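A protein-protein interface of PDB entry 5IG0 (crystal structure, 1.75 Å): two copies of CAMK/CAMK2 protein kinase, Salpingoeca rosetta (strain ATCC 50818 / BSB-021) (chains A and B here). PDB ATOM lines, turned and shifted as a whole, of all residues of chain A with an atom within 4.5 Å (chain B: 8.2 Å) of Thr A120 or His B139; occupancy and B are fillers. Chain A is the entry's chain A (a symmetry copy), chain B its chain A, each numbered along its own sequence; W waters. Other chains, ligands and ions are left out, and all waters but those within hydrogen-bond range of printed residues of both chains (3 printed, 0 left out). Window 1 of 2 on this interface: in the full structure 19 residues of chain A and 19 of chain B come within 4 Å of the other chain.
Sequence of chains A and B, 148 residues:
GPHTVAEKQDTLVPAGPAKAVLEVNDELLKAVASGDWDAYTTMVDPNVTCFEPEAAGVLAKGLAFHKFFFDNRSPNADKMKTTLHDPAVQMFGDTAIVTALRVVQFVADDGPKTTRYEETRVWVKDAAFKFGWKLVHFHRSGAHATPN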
ATOM      1  N   ILE A  97      31.319  -3.670   8.169  1.00  0.00           N
ATOM      2  CA  ILE A  97      30.077  -3.923   7.447  1.00  0.00           C
ATOM      3  C   ILE A  97      30.429  -4.452   6.070  1.00  0.00           C
ATOM      4  O   ILE A  97      30.963  -3.718   5.246  1.00  0.00           O
ATOM      5  CB  ILE A  97      29.212  -2.655   7.313  1.00  0.00           C
ATOM      6  CG1 ILE A  97      28.935  -2.048   8.693  1.00  0.00           C
ATOM      7  CG2 ILE A  97      27.898  -2.982   6.606  1.00  0.00           C
ATOM      8  CD1 ILE A  97      28.274  -0.695   8.634  1.00  0.00           C
ATOM      9  N   VAL A  98      30.149  -5.732   5.837  1.00  0.00           N
ATOM     10  CA  VAL A  98      30.395  -6.348   4.541  1.00  0.00           C
ATOM     11  C   VAL A  98      29.091  -6.383   3.762  1.00  0.00           C
ATOM     12  O   VAL A  98      28.082  -6.893   4.254  1.00  0.00           O
ATOM     13  CB  VAL A  98      30.946  -7.786   4.668  1.00  0.00           C
ATOM     14  CG1 VAL A  98      31.161  -8.410   3.290  1.00  0.00           C
ATOM     15  CG2 VAL A  98      32.247  -7.796   5.454  1.00  0.00           C
ATOM     16  N   THR A  99      29.121  -5.839   2.553  1.00  0.00           N
ATOM     17  CA  THR A  99      27.964  -5.881   1.669  1.00  0.00           C
ATOM     18  C   THR A  99      28.327  -6.665   0.420  1.00  0.00           C
ATOM     19  O   THR A  99      29.463  -6.622  -0.038  1.00  0.00           O
ATOM     20  CB  THR A  99      27.486  -4.466   1.300  1.00  0.00           C
ATOM     21  OG1 THR A  99      28.578  -3.704   0.772  1.00  0.00           O
ATOM     22  CG2 THR A  99      26.938  -3.759   2.531  1.00  0.00           C
ATOM     23  N   GLU A 118      20.533  -9.594  -1.882  1.00  0.00           N
ATOM     24  CA  GLU A 118      21.346  -8.558  -1.252  1.00  0.00           C
ATOM     25  C   GLU A 118      21.734  -9.042   0.133  1.00  0.00           C
ATOM     26  O   GLU A 118      20.888  -9.560   0.849  1.00  0.00           O
ATOM     27  CB  GLU A 118      20.575  -7.245  -1.145  1.00  0.00           C
ATOM     28  CG  GLU A 118      20.075  -6.697  -2.472  1.00  0.00           C
ATOM     29  CD  GLU A 118      19.024  -5.612  -2.296  1.00  0.00           C
ATOM     30  OE1 GLU A 118      18.401  -5.546  -1.214  1.00  0.00           O
ATOM     31  OE2 GLU A 118      18.817  -4.824  -3.241  1.00  0.00           O
ATOM     32  N   GLU A 119      23.000  -8.869   0.520  1.00  0.00           N
ATOM     33  CA  GLU A 119      23.457  -9.325   1.832  1.00  0.00           C
ATOM     34  C   GLU A 119      24.245  -8.261   2.569  1.00  0.00           C
ATOM     35  O   GLU A 119      25.212  -7.720   2.035  1.00  0.00           O
ATOM     36  CB  GLU A 119      24.332 -10.577   1.712  1.00  0.00           C
ATOM     37  CG  GLU A 119      23.572 -11.890   1.595  1.00  0.00           C
ATOM     38  CD  GLU A 119      24.338 -13.066   2.189  1.00  0.00           C
ATOM     39  OE1 GLU A 119      25.581 -13.105   2.062  1.00  0.00           O
ATOM     40  OE2 GLU A 119      23.699 -13.948   2.796  1.00  0.00           O
ATOM     41  N   THR A 120      23.813  -7.977   3.796  1.00  0.00           N
ATOM     42  CA  THR A 120      24.594  -7.191   4.745  1.00  0.00           C
ATOM     43  C   THR A 120      25.090  -8.124   5.845  1.00  0.00           C
ATOM     44  O   THR A 120      24.301  -8.846   6.444  1.00  0.00           O
ATOM     45  CB  THR A 120      23.770  -6.060   5.384  1.00  0.00           C
ATOM     46  OG1 THR A 120      23.311  -5.151   4.377  1.00  0.00           O
ATOM     47  CG2 THR A 120      24.610  -5.291   6.400  1.00  0.00           C
ATOM     48  N   ARG A 121      26.395  -8.109   6.103  1.00  0.00           N
ATOM     49  CA  ARG A 121      26.985  -8.909   7.171  1.00  0.00           C
ATOM     50  C   ARG A 121      27.772  -7.996   8.093  1.00  0.00           C
ATOM     51  O   ARG A 121      28.689  -7.314   7.642  1.00  0.00           O
ATOM     52  CB  ARG A 121      27.898  -9.993   6.604  1.00  0.00           C
ATOM     53  CG  ARG A 121      27.192 -11.018   5.728  1.00  0.00           C
ATOM     54  CD  ARG A 121      27.187 -12.383   6.389  1.00  0.00           C
ATOM     55  NE  ARG A 121      26.804 -13.440   5.457  1.00  0.00           N
ATOM     56  CZ  ARG A 121      26.164 -14.556   5.798  1.00  0.00           C
ATOM     57  NH1 ARG A 121      25.815 -14.781   7.058  1.00  0.00           N
ATOM     58  NH2 ARG A 121      25.863 -15.453   4.868  1.00  0.00           N
ATOM     59  N   VAL A 122      27.414  -7.984   9.371  1.00  0.00           N
ATOM     60  CA  VAL A 122      28.100  -7.140  10.349  1.00  0.00           C
ATOM     61  C   VAL A 122      29.042  -7.990  11.187  1.00  0.00           C
ATOM     62  O   VAL A 122      28.603  -8.852  11.950  1.00  0.00           O
ATOM     63  CB  VAL A 122      27.119  -6.410  11.285  1.00  0.00           C
ATOM     64  CG1 VAL A 122      27.874  -5.405  12.157  1.00  0.00           C
ATOM     65  CG2 VAL A 122      26.040  -5.703  10.479  1.00  0.00           C
ATOM     66  N   HIS A 137      25.492 -10.024  13.220  1.00  0.00           N
ATOM     67  CA  HIS A 137      24.204  -9.790  12.573  1.00  0.00           C
ATOM     68  C   HIS A 137      24.321  -9.864  11.061  1.00  0.00           C
ATOM     69  O   HIS A 137      25.325  -9.440  10.487  1.00  0.00           O
ATOM     70  CB  HIS A 137      23.639  -8.425  12.965  1.00  0.00           C
ATOM     71  CG  HIS A 137      22.383  -8.061  12.234  1.00  0.00           C
ATOM     72  ND1 HIS A 137      21.145  -8.565  12.582  1.00  0.00           N
ATOM     73  CD2 HIS A 137      22.173  -7.258  11.166  1.00  0.00           C
ATOM     74  CE1 HIS A 137      20.231  -8.080  11.764  1.00  0.00           C
ATOM     75  NE2 HIS A 137      20.825  -7.286  10.893  1.00  0.00           N
ATOM     76  N   PHE A 138      23.297 -10.395  10.401  1.00  0.00           N
ATOM     77  CA  PHE A 138      23.251 -10.280   8.954  1.00  0.00           C
ATOM     78  C   PHE A 138      21.821 -10.159   8.452  1.00  0.00           C
ATOM     79  O   PHE A 138      20.866 -10.480   9.151  1.00  0.00           O
ATOM     80  CB  PHE A 138      23.988 -11.452   8.286  1.00  0.00           C
ATOM     81  CG  PHE A 138      23.316 -12.795   8.433  1.00  0.00           C
ATOM     82  CD1 PHE A 138      23.571 -13.598   9.534  1.00  0.00           C
ATOM     83  CD2 PHE A 138      22.482 -13.279   7.437  1.00  0.00           C
ATOM     84  CE1 PHE A 138      22.978 -14.844   9.656  1.00  0.00           C
ATOM     85  CE2 PHE A 138      21.883 -14.520   7.557  1.00  0.00           C
ATOM     86  CZ  PHE A 138      22.135 -15.304   8.664  1.00  0.00           C
ATOM     87  N   HIS A 139      21.709  -9.632   7.244  1.00  0.00           N
ATOM     88  CA  HIS A 139      20.429  -9.318   6.624  1.00  0.00           C
ATOM     89  C   HIS A 139      20.536  -9.773   5.182  1.00  0.00           C
ATOM     90  O   HIS A 139      21.353  -9.249   4.437  1.00  0.00           O
ATOM     91  CB  HIS A 139      20.158  -7.818   6.733  1.00  0.00           C
ATOM     92  CG  HIS A 139      18.766  -7.404   6.358  1.00  0.00           C
ATOM     93  ND1 HIS A 139      18.002  -8.088   5.435  1.00  0.00           N
ATOM     94  CD2 HIS A 139      18.011  -6.365   6.778  1.00  0.00           C
ATOM     95  CE1 HIS A 139      16.835  -7.482   5.308  1.00  0.00           C
ATOM     96  NE2 HIS A 139      16.809  -6.437   6.107  1.00  0.00           N
ATOM     97  N   SER A 141      18.191 -10.586   1.703  1.00  0.00           N
ATOM     98  CA  SER A 141      16.883 -10.432   1.083  1.00  0.00           C
ATOM     99  C   SER A 141      16.924 -10.758  -0.396  1.00  0.00           C
ATOM    100  O   SER A 141      17.886 -10.431  -1.089  1.00  0.00           O
ATOM    101  CB  SER A 141      16.367  -9.017   1.291  1.00  0.00           C
ATOM    102  OG  SER A 141      17.221  -8.075   0.679  1.00  0.00           O
ATOM    103  N   THR B  49      25.630   4.099   3.051  1.00  0.00           N
ATOM    104  CA  THR B  49      25.341   3.107   2.017  1.00  0.00           C
ATOM    105  C   THR B  49      24.026   2.418   2.335  1.00  0.00           C
ATOM    106  O   THR B  49      23.587   2.406   3.480  1.00  0.00           O
ATOM    107  CB  THR B  49      26.446   2.041   1.897  1.00  0.00           C
ATOM    108  OG1 THR B  49      26.603   1.361   3.151  1.00  0.00           O
ATOM    109  CG2 THR B  49      27.765   2.681   1.479  1.00  0.00           C
ATOM    110  N   CYS B  50      23.380   1.837   1.331  1.00  0.00           N
ATOM    111  CA  CYS B  50      22.167   1.102   1.627  1.00  0.00           C
ATOM    112  C   CYS B  50      21.746   0.112   0.555  1.00  0.00           C
ATOM    113  O   CYS B  50      22.063   0.267  -0.626  1.00  0.00           O
ATOM    114  CB  CYS B  50      21.021   2.081   1.884  1.00  0.00           C
ATOM    115  SG  CYS B  50      20.424   2.939   0.418  1.00  0.00           S
ATOM    116  N   PHE B  51      21.057  -0.928   1.017  1.00  0.00           N
ATOM    117  CA  PHE B  51      20.237  -1.784   0.170  1.00  0.00           C
ATOM    118  C   PHE B  51      18.788  -1.416   0.454  1.00  0.00           C
ATOM    119  O   PHE B  51      18.369  -1.425   1.609  1.00  0.00           O
ATOM    120  CB  PHE B  51      20.449  -3.272   0.469  1.00  0.00           C
ATOM    121  CG  PHE B  51      21.763  -3.836  -0.007  1.00  0.00           C
ATOM    122  CD1 PHE B  51      22.098  -3.826  -1.350  1.00  0.00           C
ATOM    123  CD2 PHE B  51      22.638  -4.430   0.890  1.00  0.00           C
ATOM    124  CE1 PHE B  51      23.289  -4.373  -1.790  1.00  0.00           C
ATOM    125  CE2 PHE B  51      23.830  -4.980   0.457  1.00  0.00           C
ATOM    126  CZ  PHE B  51      24.157  -4.949  -0.882  1.00  0.00           C
ATOM    127  N   GLU B  52      18.021  -1.091  -0.580  1.00  0.00           N
ATOM    128  CA  GLU B  52      16.598  -0.810  -0.407  1.00  0.00           C
ATOM    129  C   GLU B  52      15.898  -1.005  -1.745  1.00  0.00           C
ATOM    130  O   GLU B  52      16.551  -0.991  -2.787  1.00  0.00           O
ATOM    131  CB  GLU B  52      16.375   0.608   0.126  1.00  0.00           C
ATOM    132  CG  GLU B  52      16.835   1.711  -0.819  1.00  0.00           C
ATOM    133  CD  GLU B  52      16.459   3.100  -0.339  1.00  0.00           C
ATOM    134  OE1 GLU B  52      16.676   4.067  -1.099  1.00  0.00           O
ATOM    135  OE2 GLU B  52      15.943   3.230   0.790  1.00  0.00           O
ATOM    136  N   PRO B  53      14.573  -1.212  -1.723  1.00  0.00           N
ATOM    137  CA  PRO B  53      13.846  -1.427  -2.981  1.00  0.00           C
ATOM    138  C   PRO B  53      14.131  -0.347  -4.027  1.00  0.00           C
ATOM    139  O   PRO B  53      14.278  -0.662  -5.209  1.00  0.00           O
ATOM    140  CB  PRO B  53      12.382  -1.397  -2.544  1.00  0.00           C
ATOM    141  CG  PRO B  53      12.411  -1.888  -1.139  1.00  0.00           C
ATOM    142  CD  PRO B  53      13.699  -1.373  -0.547  1.00  0.00           C
ATOM    143  N   LEU B  59      23.963  -1.795  -4.136  1.00  0.00           N
ATOM    144  CA  LEU B  59      24.253  -0.904  -3.024  1.00  0.00           C
ATOM    145  C   LEU B  59      24.333   0.542  -3.486  1.00  0.00           C
ATOM    146  O   LEU B  59      25.167   0.885  -4.326  1.00  0.00           O
ATOM    147  CB  LEU B  59      25.570  -1.304  -2.358  1.00  0.00           C
ATOM    148  CG  LEU B  59      25.848  -0.636  -1.018  1.00  0.00           C
ATOM    149  CD1 LEU B  59      25.039  -1.308   0.072  1.00  0.00           C
ATOM    150  CD2 LEU B  59      27.339  -0.672  -0.702  1.00  0.00           C
ATOM    151  N   ILE B  97      23.320  -1.622  16.238  1.00  0.00           N
ATOM    152  CA  ILE B  97      22.542  -2.263  15.184  1.00  0.00           C
ATOM    153  C   ILE B  97      21.080  -2.225  15.585  1.00  0.00           C
ATOM    154  O   ILE B  97      20.682  -2.899  16.530  1.00  0.00           O
ATOM    155  CB  ILE B  97      22.979  -3.721  14.942  1.00  0.00           C
ATOM    156  CG1 ILE B  97      24.478  -3.787  14.637  1.00  0.00           C
ATOM    157  CG2 ILE B  97      22.179  -4.328  13.791  1.00  0.00           C
ATOM    158  CD1 ILE B  97      25.024  -5.191  14.593  1.00  0.00           C
ATOM    159  N   VAL B  98      20.292  -1.417  14.880  1.00  0.00           N
ATOM    160  CA  VAL B  98      18.862  -1.325  15.134  1.00  0.00           C
ATOM    161  C   VAL B  98      18.130  -2.191  14.123  1.00  0.00           C
ATOM    162  O   VAL B  98      18.324  -2.041  12.915  1.00  0.00           O
ATOM    163  CB  VAL B  98      18.338   0.125  15.031  1.00  0.00           C
ATOM    164  CG1 VAL B  98      16.830   0.177  15.273  1.00  0.00           C
ATOM    165  CG2 VAL B  98      19.057   1.027  16.020  1.00  0.00           C
ATOM    166  N   THR B  99      17.294  -3.091  14.624  1.00  0.00           N
ATOM    167  CA  THR B  99      16.468  -3.926  13.765  1.00  0.00           C
ATOM    168  C   THR B  99      15.005  -3.628  14.047  1.00  0.00           C
ATOM    169  O   THR B  99      14.634  -3.333  15.177  1.00  0.00           O
ATOM    170  CB  THR B  99      16.766  -5.421  13.976  1.00  0.00           C
ATOM    171  OG1 THR B  99      16.654  -5.749  15.365  1.00  0.00           O
ATOM    172  CG2 THR B  99      18.174  -5.747  13.501  1.00  0.00           C
ATOM    173  N   ALA B 100      14.176  -3.687  13.013  1.00  0.00           N
ATOM    174  CA  ALA B 100      12.761  -3.402  13.176  1.00  0.00           C
ATOM    175  C   ALA B 100      11.977  -3.883  11.973  1.00  0.00           C
ATOM    176  O   ALA B 100      12.552  -4.191  10.926  1.00  0.00           O
ATOM    177  CB  ALA B 100      12.542  -1.911  13.385  1.00  0.00           C
ATOM    178  N   TYR B 117       8.248  -4.403   5.755  1.00  0.00           N
ATOM    179  CA  TYR B 117       9.662  -4.488   5.413  1.00  0.00           C
ATOM    180  C   TYR B 117      10.486  -4.868   6.634  1.00  0.00           C
ATOM    181  O   TYR B 117      10.196  -4.421   7.743  1.00  0.00           O
ATOM    182  CB  TYR B 117      10.177  -3.156   4.871  1.00  0.00           C
ATOM    183  CG  TYR B 117       9.451  -2.652   3.651  1.00  0.00           C
ATOM    184  CD1 TYR B 117       8.306  -1.879   3.773  1.00  0.00           C
ATOM    185  CD2 TYR B 117       9.920  -2.937   2.378  1.00  0.00           C
ATOM    186  CE1 TYR B 117       7.640  -1.413   2.655  1.00  0.00           C
ATOM    187  CE2 TYR B 117       9.264  -2.474   1.257  1.00  0.00           C
ATOM    188  CZ  TYR B 117       8.125  -1.714   1.402  1.00  0.00           C
ATOM    189  OH  TYR B 117       7.472  -1.252   0.286  1.00  0.00           O
ATOM    190  N   GLU B 118      11.506  -5.692   6.424  1.00  0.00           N
ATOM    191  CA  GLU B 118      12.548  -5.908   7.423  1.00  0.00           C
ATOM    192  C   GLU B 118      13.575  -4.799   7.282  1.00  0.00           C
ATOM    193  O   GLU B 118      13.968  -4.482   6.167  1.00  0.00           O
ATOM    194  CB  GLU B 118      13.222  -7.265   7.231  1.00  0.00           C
ATOM    195  CG  GLU B 118      12.274  -8.452   7.285  1.00  0.00           C
ATOM    196  CD  GLU B 118      12.902  -9.724   6.737  1.00  0.00           C
ATOM    197  OE1 GLU B 118      13.888  -9.630   5.975  1.00  0.00           O
ATOM    198  OE2 GLU B 118      12.409 -10.822   7.067  1.00  0.00           O
ATOM    199  N   GLU B 119      14.018  -4.216   8.397  1.00  0.00           N
ATOM    200  CA  GLU B 119      14.993  -3.127   8.344  1.00  0.00           C
ATOM    201  C   GLU B 119      16.141  -3.334   9.310  1.00  0.00           C
ATOM    202  O   GLU B 119      15.924  -3.544  10.500  1.00  0.00           O
ATOM    203  CB  GLU B 119      14.337  -1.778   8.656  1.00  0.00           C
ATOM    204  CG  GLU B 119      13.630  -1.114   7.484  1.00  0.00           C
ATOM    205  CD  GLU B 119      13.645   0.407   7.576  1.00  0.00           C
ATOM    206  OE1 GLU B 119      13.534   0.946   8.698  1.00  0.00           O
ATOM    207  OE2 GLU B 119      13.779   1.067   6.527  1.00  0.00           O
ATOM    208  N   THR B 120      17.358  -3.271   8.772  1.00  0.00           N
ATOM    209  CA  THR B 120      18.572  -3.175   9.576  1.00  0.00           C
ATOM    210  C   THR B 120      19.144  -1.770   9.414  1.00  0.00           C
ATOM    211  O   THR B 120      19.340  -1.310   8.296  1.00  0.00           O
ATOM    212  CB  THR B 120      19.638  -4.200   9.150  1.00  0.00           C
ATOM    213  OG1 THR B 120      19.139  -5.532   9.315  1.00  0.00           O
ATOM    214  CG2 THR B 120      20.905  -4.038   9.985  1.00  0.00           C
ATOM    215  N   ARG B 121      19.402  -1.094  10.531  1.00  0.00           N
ATOM    216  CA  ARG B 121      20.006   0.234  10.512  1.00  0.00           C
ATOM    217  C   ARG B 121      21.251   0.220  11.377  1.00  0.00           C
ATOM    218  O   ARG B 121      21.170  -0.093  12.563  1.00  0.00           O
ATOM    219  CB  ARG B 121      19.026   1.289  11.021  1.00  0.00           C
ATOM    220  CG  ARG B 121      17.772   1.447  10.174  1.00  0.00           C
ATOM    221  CD  ARG B 121      17.749   2.800   9.488  1.00  0.00           C
ATOM    222  NE  ARG B 121      16.435   3.106   8.929  1.00  0.00           N
ATOM    223  CZ  ARG B 121      16.227   3.847   7.844  1.00  0.00           C
ATOM    224  NH1 ARG B 121      17.246   4.369   7.172  1.00  0.00           N
ATOM    225  NH2 ARG B 121      14.989   4.063   7.420  1.00  0.00           N
ATOM    226  N   VAL B 122      22.393   0.554  10.788  1.00  0.00           N
ATOM    227  CA  VAL B 122      23.657   0.572  11.523  1.00  0.00           C
ATOM    228  C   VAL B 122      24.038   2.008  11.850  1.00  0.00           C
ATOM    229  O   VAL B 122      24.325   2.803  10.953  1.00  0.00           O
ATOM    230  CB  VAL B 122      24.805  -0.083  10.735  1.00  0.00           C
ATOM    231  CG1 VAL B 122      26.048  -0.205  11.618  1.00  0.00           C
ATOM    232  CG2 VAL B 122      24.386  -1.453  10.224  1.00  0.00           C
ATOM    233  N   LEU B 135      23.818   7.612  10.921  1.00  0.00           N
ATOM    234  CA  LEU B 135      23.481   6.405  10.177  1.00  0.00           C
ATOM    235  C   LEU B 135      24.512   6.179   9.072  1.00  0.00           C
ATOM    236  O   LEU B 135      24.708   7.052   8.229  1.00  0.00           O
ATOM    237  CB  LEU B 135      22.076   6.524   9.583  1.00  0.00           C
ATOM    238  CG  LEU B 135      21.585   5.317   8.783  1.00  0.00           C
ATOM    239  CD1 LEU B 135      21.379   4.132   9.702  1.00  0.00           C
ATOM    240  CD2 LEU B 135      20.307   5.660   8.034  1.00  0.00           C
ATOM    241  N   HIS B 137      24.883   2.845   7.439  1.00  0.00           N
ATOM    242  CA  HIS B 137      24.389   1.824   6.519  1.00  0.00           C
ATOM    243  C   HIS B 137      23.008   1.338   6.920  1.00  0.00           C
ATOM    244  O   HIS B 137      22.702   1.223   8.107  1.00  0.00           O
ATOM    245  CB  HIS B 137      25.344   0.631   6.469  1.00  0.00           C
ATOM    246  CG  HIS B 137      24.834  -0.514   5.648  1.00  0.00           C
ATOM    247  ND1 HIS B 137      24.899  -0.528   4.270  1.00  0.00           N
ATOM    248  CD2 HIS B 137      24.238  -1.674   6.007  1.00  0.00           C
ATOM    249  CE1 HIS B 137      24.371  -1.651   3.820  1.00  0.00           C
ATOM    250  NE2 HIS B 137      23.959  -2.365   4.851  1.00  0.00           N
ATOM    251  N   PHE B 138      22.163   1.043   5.936  1.00  0.00           N
ATOM    252  CA  PHE B 138      20.921   0.359   6.253  1.00  0.00           C
ATOM    253  C   PHE B 138      20.505  -0.579   5.131  1.00  0.00           C
ATOM    254  O   PHE B 138      20.969  -0.475   4.001  1.00  0.00           O
ATOM    255  CB  PHE B 138      19.810   1.365   6.591  1.00  0.00           C
ATOM    256  CG  PHE B 138      19.327   2.198   5.429  1.00  0.00           C
ATOM    257  CD1 PHE B 138      19.954   3.390   5.102  1.00  0.00           C
ATOM    258  CD2 PHE B 138      18.207   1.817   4.706  1.00  0.00           C
ATOM    259  CE1 PHE B 138      19.493   4.170   4.055  1.00  0.00           C
ATOM    260  CE2 PHE B 138      17.746   2.589   3.655  1.00  0.00           C
ATOM    261  CZ  PHE B 138      18.387   3.768   3.333  1.00  0.00           C
ATOM    262  N   HIS B 139      19.660  -1.529   5.498  1.00  0.00           N
ATOM    263  CA  HIS B 139      19.227  -2.600   4.612  1.00  0.00           C
ATOM    264  C   HIS B 139      17.737  -2.757   4.837  1.00  0.00           C
ATOM    265  O   HIS B 139      17.320  -3.105   5.934  1.00  0.00           O
ATOM    266  CB  HIS B 139      19.995  -3.881   4.939  1.00  0.00           C
ATOM    267  CG  HIS B 139      19.823  -4.987   3.940  1.00  0.00           C
ATOM    268  ND1 HIS B 139      18.679  -5.147   3.186  1.00  0.00           N
ATOM    269  CD2 HIS B 139      20.652  -5.993   3.586  1.00  0.00           C
ATOM    270  CE1 HIS B 139      18.818  -6.206   2.410  1.00  0.00           C
ATOM    271  NE2 HIS B 139      20.002  -6.740   2.627  1.00  0.00           N
ATOM    272  N   ARG B 140      16.939  -2.449   3.817  1.00  0.00           N
ATOM    273  CA  ARG B 140      15.495  -2.599   3.887  1.00  0.00           C
ATOM    274  C   ARG B 140      15.052  -3.562   2.799  1.00  0.00           C
ATOM    275  O   ARG B 140      15.466  -3.436   1.645  1.00  0.00           O
ATOM    276  CB  ARG B 140      14.776  -1.257   3.724  1.00  0.00           C
ATOM    277  CG  ARG B 140      13.261  -1.417   3.632  1.00  0.00           C
ATOM    278  CD  ARG B 140      12.499  -0.119   3.870  1.00  0.00           C
ATOM    279  NE  ARG B 140      12.785   0.906   2.868  1.00  0.00           N
ATOM    280  CZ  ARG B 140      13.454   2.037   3.097  1.00  0.00           C
ATOM    281  NH1 ARG B 140      13.922   2.328   4.303  1.00  0.00           N
ATOM    282  NH2 ARG B 140      13.650   2.891   2.104  1.00  0.00           N
ATOM    283  N   SER B 141      14.225  -4.534   3.169  1.00  0.00           N
ATOM    284  CA  SER B 141      13.720  -5.490   2.195  1.00  0.00           C
ATOM    285  C   SER B 141      12.252  -5.794   2.420  1.00  0.00           C
ATOM    286  O   SER B 141      11.797  -5.898   3.558  1.00  0.00           O
ATOM    287  CB  SER B 141      14.533  -6.774   2.248  1.00  0.00           C
ATOM    288  OG  SER B 141      14.423  -7.386   3.516  1.00  0.00           O
ATOM    289  N   GLY B 142      11.525  -5.946   1.317  1.00  0.00           N
ATOM    290  CA  GLY B 142      10.088  -6.145   1.354  1.00  0.00           C
ATOM    291  C   GLY B 142       9.690  -7.594   1.535  1.00  0.00           C
ATOM    292  O   GLY B 142      10.466  -8.506   1.253  1.00  0.00           O
HETATM  293  O   HOH W   1      16.161  -4.150  -0.895  1.00  0.00           O
HETATM  294  O   HOH W   2      19.575  -2.129  -2.989  1.00  0.00           O
HETATM  295  O   HOH W   3      16.887  -3.243  -4.323  1.00  0.00           O
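A ring nitrogen (NE2) of His A139 is in hydrogen-bond range of the backbone carbonyl oxygen of Glu B118 (3.4 Å).
NE2 of His B139 sits at hydrogen-bond distance from O of Glu A118.
A ring nitrogen (NE2) of His A137 sits at hydrogen-bond distance from the side-chain hydroxyl (OG1) of Thr B120.
A ring nitrogen (NE2) of His B137 sits at hydrogen-bond distance from the side-chain hydroxyl (OG1) of Thr A120 (2.9 Å).
A ring nitrogen (NE2) of His B139 lies within hydrogen-bond range of the backbone carbonyl oxygen (O) of His A139, 3.4 Å away.
Of the printed residues of chain B, Thr A120 touches Phe B51 (3.6 Å), His B137 (2.9 Å) and His B139 (2.9 Å).
Of the printed residues of chain B, His A139 touches Glu B118, Thr B120, His B139 and Ser B141.
Of the printed residues of chain A, Leu B59 touches Thr A99.
Of the printed residues of chain A, Thr B120 touches His A137 (2.9 Å) and His A139 (2.9 Å).
Of the printed residues of chain A, His B137 touches Ile A97 (3.9 Å), Thr A99 (3.6 Å) and Thr A120 (2.9 Å).
The nearest residue of chain B that does not touch Thr A120 is Phe B138 (5.2 Å).
The nearest residue of chain A that does not touch His B139 is Glu A119 (4.2 Å).
Water W1 lies within hydrogen-bond range of the side-chain carboxylate (OE1) of Glu A118 (2.7 Å) and the backbone carbonyl oxygen (O) of Arg B140 (2.7 Å).
Water W3 lies within hydrogen-bond range of OE2 of Glu A118 (2.7 Å) and O of Glu B52 (2.7 Å).
Water W2 lies within hydrogen-bond range of the side-chain carboxylate of Glu A118 (2.8 Å) and the backbone NH of Glu B52 (3.0 Å).
Glu A118 touches His B139, and with the chains exchanged His A139 touches Glu B118.
Thr A120 touches His B139, and with the chains exchanged His A139 touches Thr B120.
His A139 touches its own counterpart, His B139.
His A139 touches Ser B141, and with the chains exchanged Ser A141 touches His B139.
Positions printed for both chains: 97, 98, 99, 118, 119, 120, 121, 122, 137, 138, 139 and 141.
The backbone NH (N) of His A139 sits at hydrogen-bond distance from the backbone carbonyl oxygen (O) of Thr A120, at 2.8 Å.
The backbone NH (N) of Phe B51 is in hydrogen-bond range of the backbone carbonyl oxygen (O) of Phe B138 (3.0 Å).
ND1 of His B137 is in hydrogen-bond range of OG1 of Thr B49.
The guanidinium group of Arg A121 lies within salt-bridge range of the side-chain carboxylate of Glu A119, 3.4 Å away.
Ile A97 touches Val B122 (CD1 to CG1, 3.8 Å).
Ile A97 touches His B137 (CD1 to CB, 3.9 Å).
Thr A99 touches Phe B51.
O of Glu A119 touches CE2 of Phe B51, 3.5 Å away.
His B139 touches Thr A120 (CD2 to OG1, 2.9 Å).
CD1 of Ile B97 touches CG1 of Val A122, 3.8 Å away.
His A137 touches Thr B99.
His A139 touches Ser B141 (CE1 to OG, 3.0 Å).
His B139 touches Ser A141.
Ser A141 touches Ser B141.
Of the 23 printed residues of chain B, 10 touch a printed residue of chain A.
Hydrophobic or aromatic side chains of chain B within 4 Å of the printed part of chain A: Phe B51, Leu B59, Ile B97, Val B122, His B137 and His B139.
Of the 12 printed residues of chain A, 9 touch a printed residue of chain B.
Printed residues of chain A that touch a printed residue of chain B: Ile A97, Thr A99, Glu A118, Glu A119, Thr A120, Val A122, His A137, His A139 and Ser A141.
Hydrophobic or aromatic side chains of chain A that line the printed part of chain B: Ile A97, Val A122, His A137 and His A139.
Along chain A the printed residues that touch a printed residue of chain B span positions 97 to 141.
Among the printed residues, no Asp or Glu carboxylate lies within 4 Å of a Lys or Arg side-chain nitrogen of the other chain.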
